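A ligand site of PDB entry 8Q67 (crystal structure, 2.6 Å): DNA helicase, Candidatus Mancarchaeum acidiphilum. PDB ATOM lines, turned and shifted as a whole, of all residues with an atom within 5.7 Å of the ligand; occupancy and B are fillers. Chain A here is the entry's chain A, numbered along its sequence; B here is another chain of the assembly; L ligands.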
ATOM      1  N   SER A 286     -12.582  -5.635   9.545  1.00  0.00           N
ATOM      2  CA  SER A 286     -13.269  -4.473   9.101  1.00  0.00           C
ATOM      3  C   SER A 286     -13.447  -4.355   7.641  1.00  0.00           C
ATOM      4  O   SER A 286     -14.170  -3.505   7.231  1.00  0.00           O
ATOM      5  CB  SER A 286     -12.534  -3.261   9.577  1.00  0.00           C
ATOM      6  OG  SER A 286     -11.191  -3.412   9.269  1.00  0.00           O
ATOM      7  N   ILE A 287     -12.795  -5.167   6.838  1.00  0.00           N
ATOM      8  CA  ILE A 287     -13.019  -5.037   5.428  1.00  0.00           C
ATOM      9  C   ILE A 287     -13.691  -6.264   4.864  1.00  0.00           C
ATOM     10  O   ILE A 287     -13.374  -7.347   5.251  1.00  0.00           O
ATOM     11  CB  ILE A 287     -11.748  -4.882   4.664  1.00  0.00           C
ATOM     12  CG1 ILE A 287     -10.795  -5.883   5.146  1.00  0.00           C
ATOM     13  CG2 ILE A 287     -11.124  -3.566   4.953  1.00  0.00           C
ATOM     14  CD1 ILE A 287      -9.745  -6.279   4.209  1.00  0.00           C
ATOM     15  N   TYR A 288     -14.624  -6.070   3.955  1.00  0.00           N
ATOM     16  CA  TYR A 288     -15.328  -7.165   3.282  1.00  0.00           C
ATOM     17  C   TYR A 288     -14.397  -7.836   2.278  1.00  0.00           C
ATOM     18  O   TYR A 288     -13.522  -7.200   1.682  1.00  0.00           O
ATOM     19  CB  TYR A 288     -16.576  -6.633   2.580  1.00  0.00           C
ATOM     20  CG  TYR A 288     -17.423  -7.666   1.864  1.00  0.00           C
ATOM     21  CD1 TYR A 288     -17.070  -8.131   0.611  1.00  0.00           C
ATOM     22  CD2 TYR A 288     -18.585  -8.156   2.441  1.00  0.00           C
ATOM     23  CE1 TYR A 288     -17.829  -9.054  -0.046  1.00  0.00           C
ATOM     24  CE2 TYR A 288     -19.364  -9.080   1.798  1.00  0.00           C
ATOM     25  CZ  TYR A 288     -18.983  -9.530   0.548  1.00  0.00           C
ATOM     26  OH  TYR A 288     -19.756 -10.455  -0.107  1.00  0.00           O
ATOM     27  N   GLY A 289     -14.467  -9.142   2.155  1.00  0.00           N
ATOM     28  CA  GLY A 289     -13.788  -9.745   1.053  1.00  0.00           C
ATOM     29  C   GLY A 289     -12.362 -10.018   1.292  1.00  0.00           C
ATOM     30  O   GLY A 289     -12.007 -10.260   2.406  1.00  0.00           O
ATOM     31  N   TYR A 290     -11.582 -10.058   0.234  1.00  0.00           N
ATOM     32  CA  TYR A 290     -10.158 -10.287   0.291  1.00  0.00           C
ATOM     33  C   TYR A 290      -9.832 -11.496   1.101  1.00  0.00           C
ATOM     34  O   TYR A 290      -8.971 -11.455   1.914  1.00  0.00           O
ATOM     35  CB  TYR A 290      -9.427  -9.082   0.890  1.00  0.00           C
ATOM     36  CG  TYR A 290      -9.455  -7.820   0.103  1.00  0.00           C
ATOM     37  CD1 TYR A 290      -8.862  -7.739  -1.108  1.00  0.00           C
ATOM     38  CD2 TYR A 290     -10.014  -6.696   0.611  1.00  0.00           C
ATOM     39  CE1 TYR A 290      -8.860  -6.569  -1.821  1.00  0.00           C
ATOM     40  CE2 TYR A 290     -10.012  -5.539  -0.108  1.00  0.00           C
ATOM     41  CZ  TYR A 290      -9.433  -5.492  -1.299  1.00  0.00           C
ATOM     42  OH  TYR A 290      -9.434  -4.350  -2.004  1.00  0.00           O
ATOM     43  N   ASP A 327      -4.732  -0.197  -6.583  1.00  0.00           N
ATOM     44  CA  ASP A 327      -5.024   1.193  -6.823  1.00  0.00           C
ATOM     45  C   ASP A 327      -5.408   1.863  -5.554  1.00  0.00           C
ATOM     46  O   ASP A 327      -5.435   1.268  -4.506  1.00  0.00           O
ATOM     47  CB  ASP A 327      -6.201   1.334  -7.777  1.00  0.00           C
ATOM     48  CG  ASP A 327      -5.980   0.626  -9.067  1.00  0.00           C
ATOM     49  OD1 ASP A 327      -6.300  -0.579  -9.135  1.00  0.00           O
ATOM     50  OD2 ASP A 327      -5.483   1.256 -10.009  1.00  0.00           O
ATOM     51  N   PRO A 328      -5.750   3.140  -5.636  1.00  0.00           N
ATOM     52  CA  PRO A 328      -6.156   3.804  -4.422  1.00  0.00           C
ATOM     53  C   PRO A 328      -7.527   3.290  -4.087  1.00  0.00           C
ATOM     54  O   PRO A 328      -8.319   3.058  -4.985  1.00  0.00           O
ATOM     55  CB  PRO A 328      -6.221   5.262  -4.833  1.00  0.00           C
ATOM     56  CG  PRO A 328      -5.327   5.359  -5.993  1.00  0.00           C
ATOM     57  CD  PRO A 328      -5.522   4.081  -6.735  1.00  0.00           C
ATOM     58  N   GLY A 329      -7.821   3.132  -2.804  1.00  0.00           N
ATOM     59  CA  GLY A 329      -9.114   2.659  -2.384  1.00  0.00           C
ATOM     60  C   GLY A 329      -9.173   1.156  -2.447  1.00  0.00           C
ATOM     61  O   GLY A 329     -10.213   0.572  -2.644  1.00  0.00           O
ATOM     62  N   SER A 330      -8.015   0.531  -2.386  1.00  0.00           N
ATOM     63  CA  SER A 330      -7.986  -0.917  -2.439  1.00  0.00           C
ATOM     64  C   SER A 330      -7.852  -1.491  -1.085  1.00  0.00           C
ATOM     65  O   SER A 330      -7.476  -2.632  -0.953  1.00  0.00           O
ATOM     66  CB  SER A 330      -6.798  -1.356  -3.244  1.00  0.00           C
ATOM     67  OG  SER A 330      -6.861  -0.827  -4.534  1.00  0.00           O
ATOM     68  N   ALA A 331      -8.135  -0.696  -0.068  1.00  0.00           N
ATOM     69  CA  ALA A 331      -8.031  -1.099   1.321  1.00  0.00           C
ATOM     70  C   ALA A 331      -6.683  -1.722   1.617  1.00  0.00           C
ATOM     71  O   ALA A 331      -6.602  -2.763   2.209  1.00  0.00           O
ATOM     72  CB  ALA A 331      -9.154  -2.041   1.712  1.00  0.00           C
ATOM     73  N   LYS A 332      -5.623  -1.068   1.130  1.00  0.00           N
ATOM     74  CA  LYS A 332      -4.264  -1.545   1.327  1.00  0.00           C
ATOM     75  C   LYS A 332      -3.692  -0.978   2.604  1.00  0.00           C
ATOM     76  O   LYS A 332      -2.967  -1.664   3.334  1.00  0.00           O
ATOM     77  CB  LYS A 332      -3.390  -1.156   0.133  1.00  0.00           C
ATOM     78  CG  LYS A 332      -3.996  -1.473  -1.218  1.00  0.00           C
ATOM     79  CD  LYS A 332      -3.295  -0.709  -2.339  1.00  0.00           C
ATOM     80  CE  LYS A 332      -2.856   0.665  -1.871  1.00  0.00           C
ATOM     81  NZ  LYS A 332      -4.009   1.510  -1.439  1.00  0.00           N
ATOM     82  N   THR A 333      -4.017   0.278   2.894  1.00  0.00           N
ATOM     83  CA  THR A 333      -3.530   0.909   4.084  1.00  0.00           C
ATOM     84  C   THR A 333      -4.228   0.327   5.283  1.00  0.00           C
ATOM     85  O   THR A 333      -3.599   0.000   6.266  1.00  0.00           O
ATOM     86  CB  THR A 333      -3.723   2.412   4.039  1.00  0.00           C
ATOM     87  OG1 THR A 333      -2.981   2.934   2.948  1.00  0.00           O
ATOM     88  CG2 THR A 333      -3.187   3.019   5.298  1.00  0.00           C
ATOM     89  N   ARG A 334      -5.542   0.193   5.171  1.00  0.00           N
ATOM     90  CA  ARG A 334      -6.363  -0.348   6.245  1.00  0.00           C
ATOM     91  C   ARG A 334      -5.967  -1.772   6.641  1.00  0.00           C
ATOM     92  O   ARG A 334      -6.028  -2.124   7.816  1.00  0.00           O
ATOM     93  CB  ARG A 334      -7.845  -0.291   5.877  1.00  0.00           C
ATOM     94  CG  ARG A 334      -8.747   0.095   7.040  1.00  0.00           C
ATOM     95  CD  ARG A 334     -10.213   0.141   6.617  1.00  0.00           C
ATOM     96  NE  ARG A 334     -10.663   1.513   6.365  1.00  0.00           N
ATOM     97  CZ  ARG A 334     -10.382   2.544   7.149  1.00  0.00           C
ATOM     98  NH1 ARG A 334      -9.656   2.371   8.245  1.00  0.00           N
ATOM     99  NH2 ARG A 334     -10.847   3.753   6.842  1.00  0.00           N
ATOM    100  N   ILE A 335      -5.581  -2.593   5.671  1.00  0.00           N
ATOM    101  CA  ILE A 335      -5.212  -3.938   5.986  1.00  0.00           C
ATOM    102  C   ILE A 335      -3.909  -3.899   6.710  1.00  0.00           C
ATOM    103  O   ILE A 335      -3.719  -4.578   7.696  1.00  0.00           O
ATOM    104  CB  ILE A 335      -5.013  -4.779   4.737  1.00  0.00           C
ATOM    105  CG1 ILE A 335      -6.345  -5.262   4.230  1.00  0.00           C
ATOM    106  CG2 ILE A 335      -4.157  -5.976   5.063  1.00  0.00           C
ATOM    107  CD1 ILE A 335      -6.237  -5.889   2.878  1.00  0.00           C
ATOM    108  N   ASP A 391       3.840   0.514   4.238  1.00  0.00           N
ATOM    109  CA  ASP A 391       2.974   1.118   3.247  1.00  0.00           C
ATOM    110  C   ASP A 391       3.840   1.889   2.289  1.00  0.00           C
ATOM    111  O   ASP A 391       4.945   2.252   2.601  1.00  0.00           O
ATOM    112  CB  ASP A 391       2.000   2.059   3.917  1.00  0.00           C
ATOM    113  CG  ASP A 391       0.784   2.274   3.109  1.00  0.00           C
ATOM    114  OD1 ASP A 391       0.776   1.838   1.977  1.00  0.00           O
ATOM    115  OD2 ASP A 391      -0.163   2.889   3.579  1.00  0.00           O
ATOM    116  N   ASN A 435       1.308   1.305  -4.331  1.00  0.00           N
ATOM    117  CA  ASN A 435       0.413   1.744  -5.375  1.00  0.00           C
ATOM    118  C   ASN A 435       1.182   1.604  -6.662  1.00  0.00           C
ATOM    119  O   ASN A 435       2.367   1.714  -6.673  1.00  0.00           O
ATOM    120  CB  ASN A 435       0.018   3.189  -5.216  1.00  0.00           C
ATOM    121  CG  ASN A 435      -0.609   3.495  -3.897  1.00  0.00           C
ATOM    122  OD1 ASN A 435      -1.784   3.422  -3.723  1.00  0.00           O
ATOM    123  ND2 ASN A 435       0.196   3.887  -2.968  1.00  0.00           N
ATOM    124  N   ILE A 479     -20.491  -4.406  -0.821  1.00  0.00           N
ATOM    125  CA  ILE A 479     -19.487  -3.620  -0.133  1.00  0.00           C
ATOM    126  C   ILE A 479     -20.116  -2.478   0.568  1.00  0.00           C
ATOM    127  O   ILE A 479     -19.890  -2.221   1.716  1.00  0.00           O
ATOM    128  CB  ILE A 479     -18.501  -3.015  -1.095  1.00  0.00           C
ATOM    129  CG1 ILE A 479     -17.519  -4.059  -1.546  1.00  0.00           C
ATOM    130  CG2 ILE A 479     -17.737  -1.923  -0.412  1.00  0.00           C
ATOM    131  CD1 ILE A 479     -16.721  -3.631  -2.728  1.00  0.00           C
ATOM    132  N   TYR A 482     -21.880  -3.447   3.657  1.00  0.00           N
ATOM    133  CA  TYR A 482     -21.000  -3.684   4.771  1.00  0.00           C
ATOM    134  C   TYR A 482     -20.538  -2.424   5.404  1.00  0.00           C
ATOM    135  O   TYR A 482     -20.633  -2.260   6.592  1.00  0.00           O
ATOM    136  CB  TYR A 482     -19.800  -4.467   4.269  1.00  0.00           C
ATOM    137  CG  TYR A 482     -18.926  -5.180   5.273  1.00  0.00           C
ATOM    138  CD1 TYR A 482     -19.284  -6.407   5.746  1.00  0.00           C
ATOM    139  CD2 TYR A 482     -17.710  -4.683   5.629  1.00  0.00           C
ATOM    140  CE1 TYR A 482     -18.470  -7.111   6.584  1.00  0.00           C
ATOM    141  CE2 TYR A 482     -16.890  -5.367   6.476  1.00  0.00           C
ATOM    142  CZ  TYR A 482     -17.278  -6.580   6.950  1.00  0.00           C
ATOM    143  OH  TYR A 482     -16.475  -7.295   7.808  1.00  0.00           O
ATOM    144  N   ILE A 483     -20.073  -1.500   4.601  1.00  0.00           N
ATOM    145  CA  ILE A 483     -19.531  -0.297   5.135  1.00  0.00           C
ATOM    146  C   ILE A 483     -20.518   0.490   5.935  1.00  0.00           C
ATOM    147  O   ILE A 483     -20.183   0.972   6.980  1.00  0.00           O
ATOM    148  CB  ILE A 483     -18.983   0.560   4.033  1.00  0.00           C
ATOM    149  CG1 ILE A 483     -17.793  -0.127   3.435  1.00  0.00           C
ATOM    150  CG2 ILE A 483     -18.549   1.891   4.572  1.00  0.00           C
ATOM    151  CD1 ILE A 483     -17.102   0.702   2.404  1.00  0.00           C
ATOM    152  N   GLN A 486     -21.163  -1.124   9.526  1.00  0.00           N
ATOM    153  CA  GLN A 486     -20.145  -0.777  10.504  1.00  0.00           C
ATOM    154  C   GLN A 486     -20.402   0.582  11.114  1.00  0.00           C
ATOM    155  O   GLN A 486     -20.379   0.722  12.301  1.00  0.00           O
ATOM    156  CB  GLN A 486     -18.776  -0.762   9.854  1.00  0.00           C
ATOM    157  CG  GLN A 486     -18.485  -1.938   8.965  1.00  0.00           C
ATOM    158  CD  GLN A 486     -17.003  -2.097   8.672  1.00  0.00           C
ATOM    159  OE1 GLN A 486     -16.296  -2.776   9.385  1.00  0.00           O
ATOM    160  NE2 GLN A 486     -16.543  -1.477   7.606  1.00  0.00           N
ATOM    161  N   GLU B 409      -5.502  10.228   6.117  1.00  0.00           N
ATOM    162  CA  GLU B 409      -6.407   9.135   6.345  1.00  0.00           C
ATOM    163  C   GLU B 409      -6.492   8.727   7.770  1.00  0.00           C
ATOM    164  O   GLU B 409      -7.523   8.757   8.352  1.00  0.00           O
ATOM    165  CB  GLU B 409      -6.026   7.997   5.468  1.00  0.00           C
ATOM    166  CG  GLU B 409      -6.746   6.702   5.753  1.00  0.00           C
ATOM    167  CD  GLU B 409      -8.179   6.772   5.335  1.00  0.00           C
ATOM    168  OE1 GLU B 409      -8.994   7.250   6.119  1.00  0.00           O
ATOM    169  OE2 GLU B 409      -8.490   6.372   4.225  1.00  0.00           O
ATOM    170  N   SER B 459      -7.071  11.054  -3.577  1.00  0.00           N
ATOM    171  CA  SER B 459      -8.116  10.132  -3.123  1.00  0.00           C
ATOM    172  C   SER B 459      -8.380  10.315  -1.631  1.00  0.00           C
ATOM    173  O   SER B 459      -9.482  10.050  -1.148  1.00  0.00           O
ATOM    174  CB  SER B 459      -7.710   8.688  -3.408  1.00  0.00           C
ATOM    175  OG  SER B 459      -6.501   8.361  -2.756  1.00  0.00           O
ATOM    176  N   ARG B 460      -7.362  10.784  -0.910  1.00  0.00           N
ATOM    177  CA  ARG B 460      -7.482  11.021   0.522  1.00  0.00           C
ATOM    178  C   ARG B 460      -8.386  12.219   0.785  1.00  0.00           C
ATOM    179  O   ARG B 460      -9.110  12.265   1.790  1.00  0.00           O
ATOM    180  CB  ARG B 460      -6.105  11.261   1.138  1.00  0.00           C
ATOM    181  CG  ARG B 460      -5.090  10.172   0.783  1.00  0.00           C
ATOM    182  CD  ARG B 460      -5.466   8.846   1.403  1.00  0.00           C
ATOM    183  NE  ARG B 460      -4.487   7.801   1.145  1.00  0.00           N
ATOM    184  CZ  ARG B 460      -4.554   6.565   1.635  1.00  0.00           C
ATOM    185  NH1 ARG B 460      -5.561   6.228   2.427  1.00  0.00           N
ATOM    186  NH2 ARG B 460      -3.621   5.673   1.337  1.00  0.00           N
ATOM    187  N   PRO B 557     -14.608   2.805  -2.989  1.00  0.00           N
ATOM    188  CA  PRO B 557     -15.557   2.804  -1.883  1.00  0.00           C
ATOM    189  C   PRO B 557     -15.349   3.896  -0.897  1.00  0.00           C
ATOM    190  O   PRO B 557     -16.175   4.108  -0.072  1.00  0.00           O
ATOM    191  CB  PRO B 557     -15.307   1.496  -1.197  1.00  0.00           C
ATOM    192  CG  PRO B 557     -14.707   0.654  -2.198  1.00  0.00           C
ATOM    193  CD  PRO B 557     -13.856   1.544  -3.003  1.00  0.00           C
ATOM    194  N   ARG B 558     -14.264   4.624  -0.979  1.00  0.00           N
ATOM    195  CA  ARG B 558     -13.957   5.681  -0.086  1.00  0.00           C
ATOM    196  C   ARG B 558     -14.793   6.930  -0.231  1.00  0.00           C
ATOM    197  O   ARG B 558     -14.804   7.743   0.638  1.00  0.00           O
ATOM    198  CB  ARG B 558     -12.478   5.888  -0.288  1.00  0.00           C
ATOM    199  CG  ARG B 558     -11.912   7.250  -0.112  1.00  0.00           C
ATOM    200  CD  ARG B 558     -10.569   7.203  -0.799  1.00  0.00           C
ATOM    201  NE  ARG B 558      -9.621   6.396  -0.072  1.00  0.00           N
ATOM    202  CZ  ARG B 558      -9.127   6.764   1.089  1.00  0.00           C
ATOM    203  NH1 ARG B 558      -9.495   7.898   1.632  1.00  0.00           N
ATOM    204  NH2 ARG B 558      -8.279   5.990   1.693  1.00  0.00           N
ATOM    205  N   GLU B 561     -17.533   6.996   2.556  1.00  0.00           N
ATOM    206  CA  GLU B 561     -17.194   7.504   3.816  1.00  0.00           C
ATOM    207  C   GLU B 561     -17.275   8.931   3.779  1.00  0.00           C
ATOM    208  O   GLU B 561     -17.691   9.495   4.719  1.00  0.00           O
ATOM    209  CB  GLU B 561     -15.821   7.125   4.149  1.00  0.00           C
ATOM    210  CG  GLU B 561     -15.749   5.708   4.544  1.00  0.00           C
ATOM    211  CD  GLU B 561     -14.371   5.329   4.910  1.00  0.00           C
ATOM    212  OE1 GLU B 561     -13.477   6.168   4.853  1.00  0.00           O
ATOM    213  OE2 GLU B 561     -14.200   4.167   5.265  1.00  0.00           O
HETATM  214  P1  LIG L   1      -5.913   3.267   0.431  1.00  0.00           P
HETATM  215  O1  LIG L   1      -5.936   3.985  -0.818  1.00  0.00           O
HETATM  216  O2  LIG L   1      -6.121   1.972  -0.168  1.00  0.00           O
HETATM  217  O3  LIG L   1      -4.629   3.375   1.080  1.00  0.00           O
HETATM  218  O4  LIG L   1      -6.232   1.417   2.299  1.00  0.00           O
HETATM  219  O5  LIG L   1      -7.432   3.207   3.774  1.00  0.00           O
HETATM  220  O6  LIG L   1      -7.027   3.621   1.383  1.00  0.00           O
HETATM  221  O7  LIG L   1      -8.661   2.034   1.818  1.00  0.00           O
HETATM  222  C1  LIG L   1      -9.799   1.861   2.649  1.00  0.00           C
HETATM  223  C2  LIG L   1     -11.034   2.341   1.942  1.00  0.00           C
HETATM  224  O8  LIG L   1     -11.786   1.309   1.343  1.00  0.00           O
HETATM  225  C3  LIG L   1     -11.887   2.829   3.033  1.00  0.00           C
HETATM  226  O9  LIG L   1     -12.600   3.854   2.435  1.00  0.00           O
HETATM  227  C4  LIG L   1     -12.780   1.648   3.374  1.00  0.00           C
HETATM  228  O10 LIG L   1     -14.030   1.993   3.951  1.00  0.00           O
HETATM  229  C5  LIG L   1     -12.988   1.042   2.039  1.00  0.00           C
HETATM  230  N1  LIG L   1     -13.324  -0.403   2.161  1.00  0.00           N
HETATM  231  C6  LIG L   1     -14.001  -1.102   3.094  1.00  0.00           C
HETATM  232  N2  LIG L   1     -14.103  -2.393   2.748  1.00  0.00           N
HETATM  233  C7  LIG L   1     -13.501  -2.524   1.566  1.00  0.00           C
HETATM  234  C8  LIG L   1     -13.179  -3.545   0.578  1.00  0.00           C
HETATM  235  N3  LIG L   1     -13.527  -4.793   0.686  1.00  0.00           N
HETATM  236  N4  LIG L   1     -12.534  -3.227  -0.515  1.00  0.00           N
HETATM  237  C9  LIG L   1     -12.123  -2.007  -0.764  1.00  0.00           C
HETATM  238  N5  LIG L   1     -12.351  -1.028   0.083  1.00  0.00           N
HETATM  239  C10 LIG L   1     -13.008  -1.220   1.207  1.00  0.00           C
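The backbone NH (N) of Lys 332 is in hydrogen-bond range of an oxygen (O4) of the ligand (2.8 Å). An oxygen (O2) of the ligand lies within salt-bridge range of the side-chain amino group (NZ) of Lys 332 (2.5 Å). O3 of the ligand is in salt-bridge range of NH2 of Arg 460 of chain B (2.5 Å). N of Thr 333 lies within hydrogen-bond range of O4 of the ligand. The side-chain hydroxyl (OG1) of Thr 333 sits at hydrogen-bond distance from an oxygen (O3) of the ligand. The side-chain carboxylate (OE2) of Glu 561 of chain B lies within hydrogen-bond range of an oxygen (O10) of the ligand (2.5 Å). O of Tyr 288 is in hydrogen-bond range of N3 of the ligand, at 2.6 Å. NH2 of Arg 558 of chain B lies within salt-bridge range of O6 of the ligand (2.7 Å). O1 of the ligand sits at hydrogen-bond distance from N of Gly 329, at 2.9 Å. The backbone NH (N) of Arg 334 sits at hydrogen-bond distance from an oxygen (O4) of the ligand. The backbone NH of Ala 331 lies within hydrogen-bond range of an oxygen (O2) of the ligand, 3.3 Å away. The backbone NH (N) of Ser 330 lies within hydrogen-bond range of an oxygen (O2) of the ligand, 3.3 Å away. OE2 of Glu 409 of chain B is in hydrogen-bond range of O5 of the ligand (3.4 Å).
The side-chain amino group (NZ) of Lys 332 is in hydrogen-bond range of the backbone carbonyl oxygen (O) of Asp 327 (3.4 Å). OG1 of Thr 333 sits at hydrogen-bond distance from NH2 of Arg 460 of chain B, at 3.2 Å. The guanidinium group (NH1) of Arg 460 of chain B is in salt-bridge range of the side-chain carboxylate (OE2) of Glu 409 of chain B (3.4 Å). The side-chain hydroxyl (OG1) of Thr 333 is in hydrogen-bond range of the side-chain carboxylate (OD2) of Asp 391 (2.9 Å). The guanidinium group of Arg 334 is in salt-bridge range of the side-chain carboxylate of Glu 561 of chain B, at 3.7 Å. NH2 of Arg 558 of chain B lies within salt-bridge range of OE2 of Glu 409 of chain B, at 2.6 Å. OH of Tyr 290 sits at hydrogen-bond distance from O of Ser 330 (2.8 Å). The side-chain hydroxyl (OG) of Ser 330 is in hydrogen-bond range of the backbone carbonyl oxygen (O) of Asp 327 (2.5 Å).
CG2 of Ile 287 touches N2 of the ligand (3.9 Å). Tyr 290 touches the ligand (CE2 to N4, 3.4 Å). Pro 328 touches the ligand. Ile 483 touches the ligand (CD1 to C6, 3.7 Å). Pro 557 of chain B touches the ligand. Hydrophobic or aromatic side chains within 4 Å of the ligand: Ile 287, Tyr 290, Ala 331, Ile 483 and Pro 557 of chain B.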
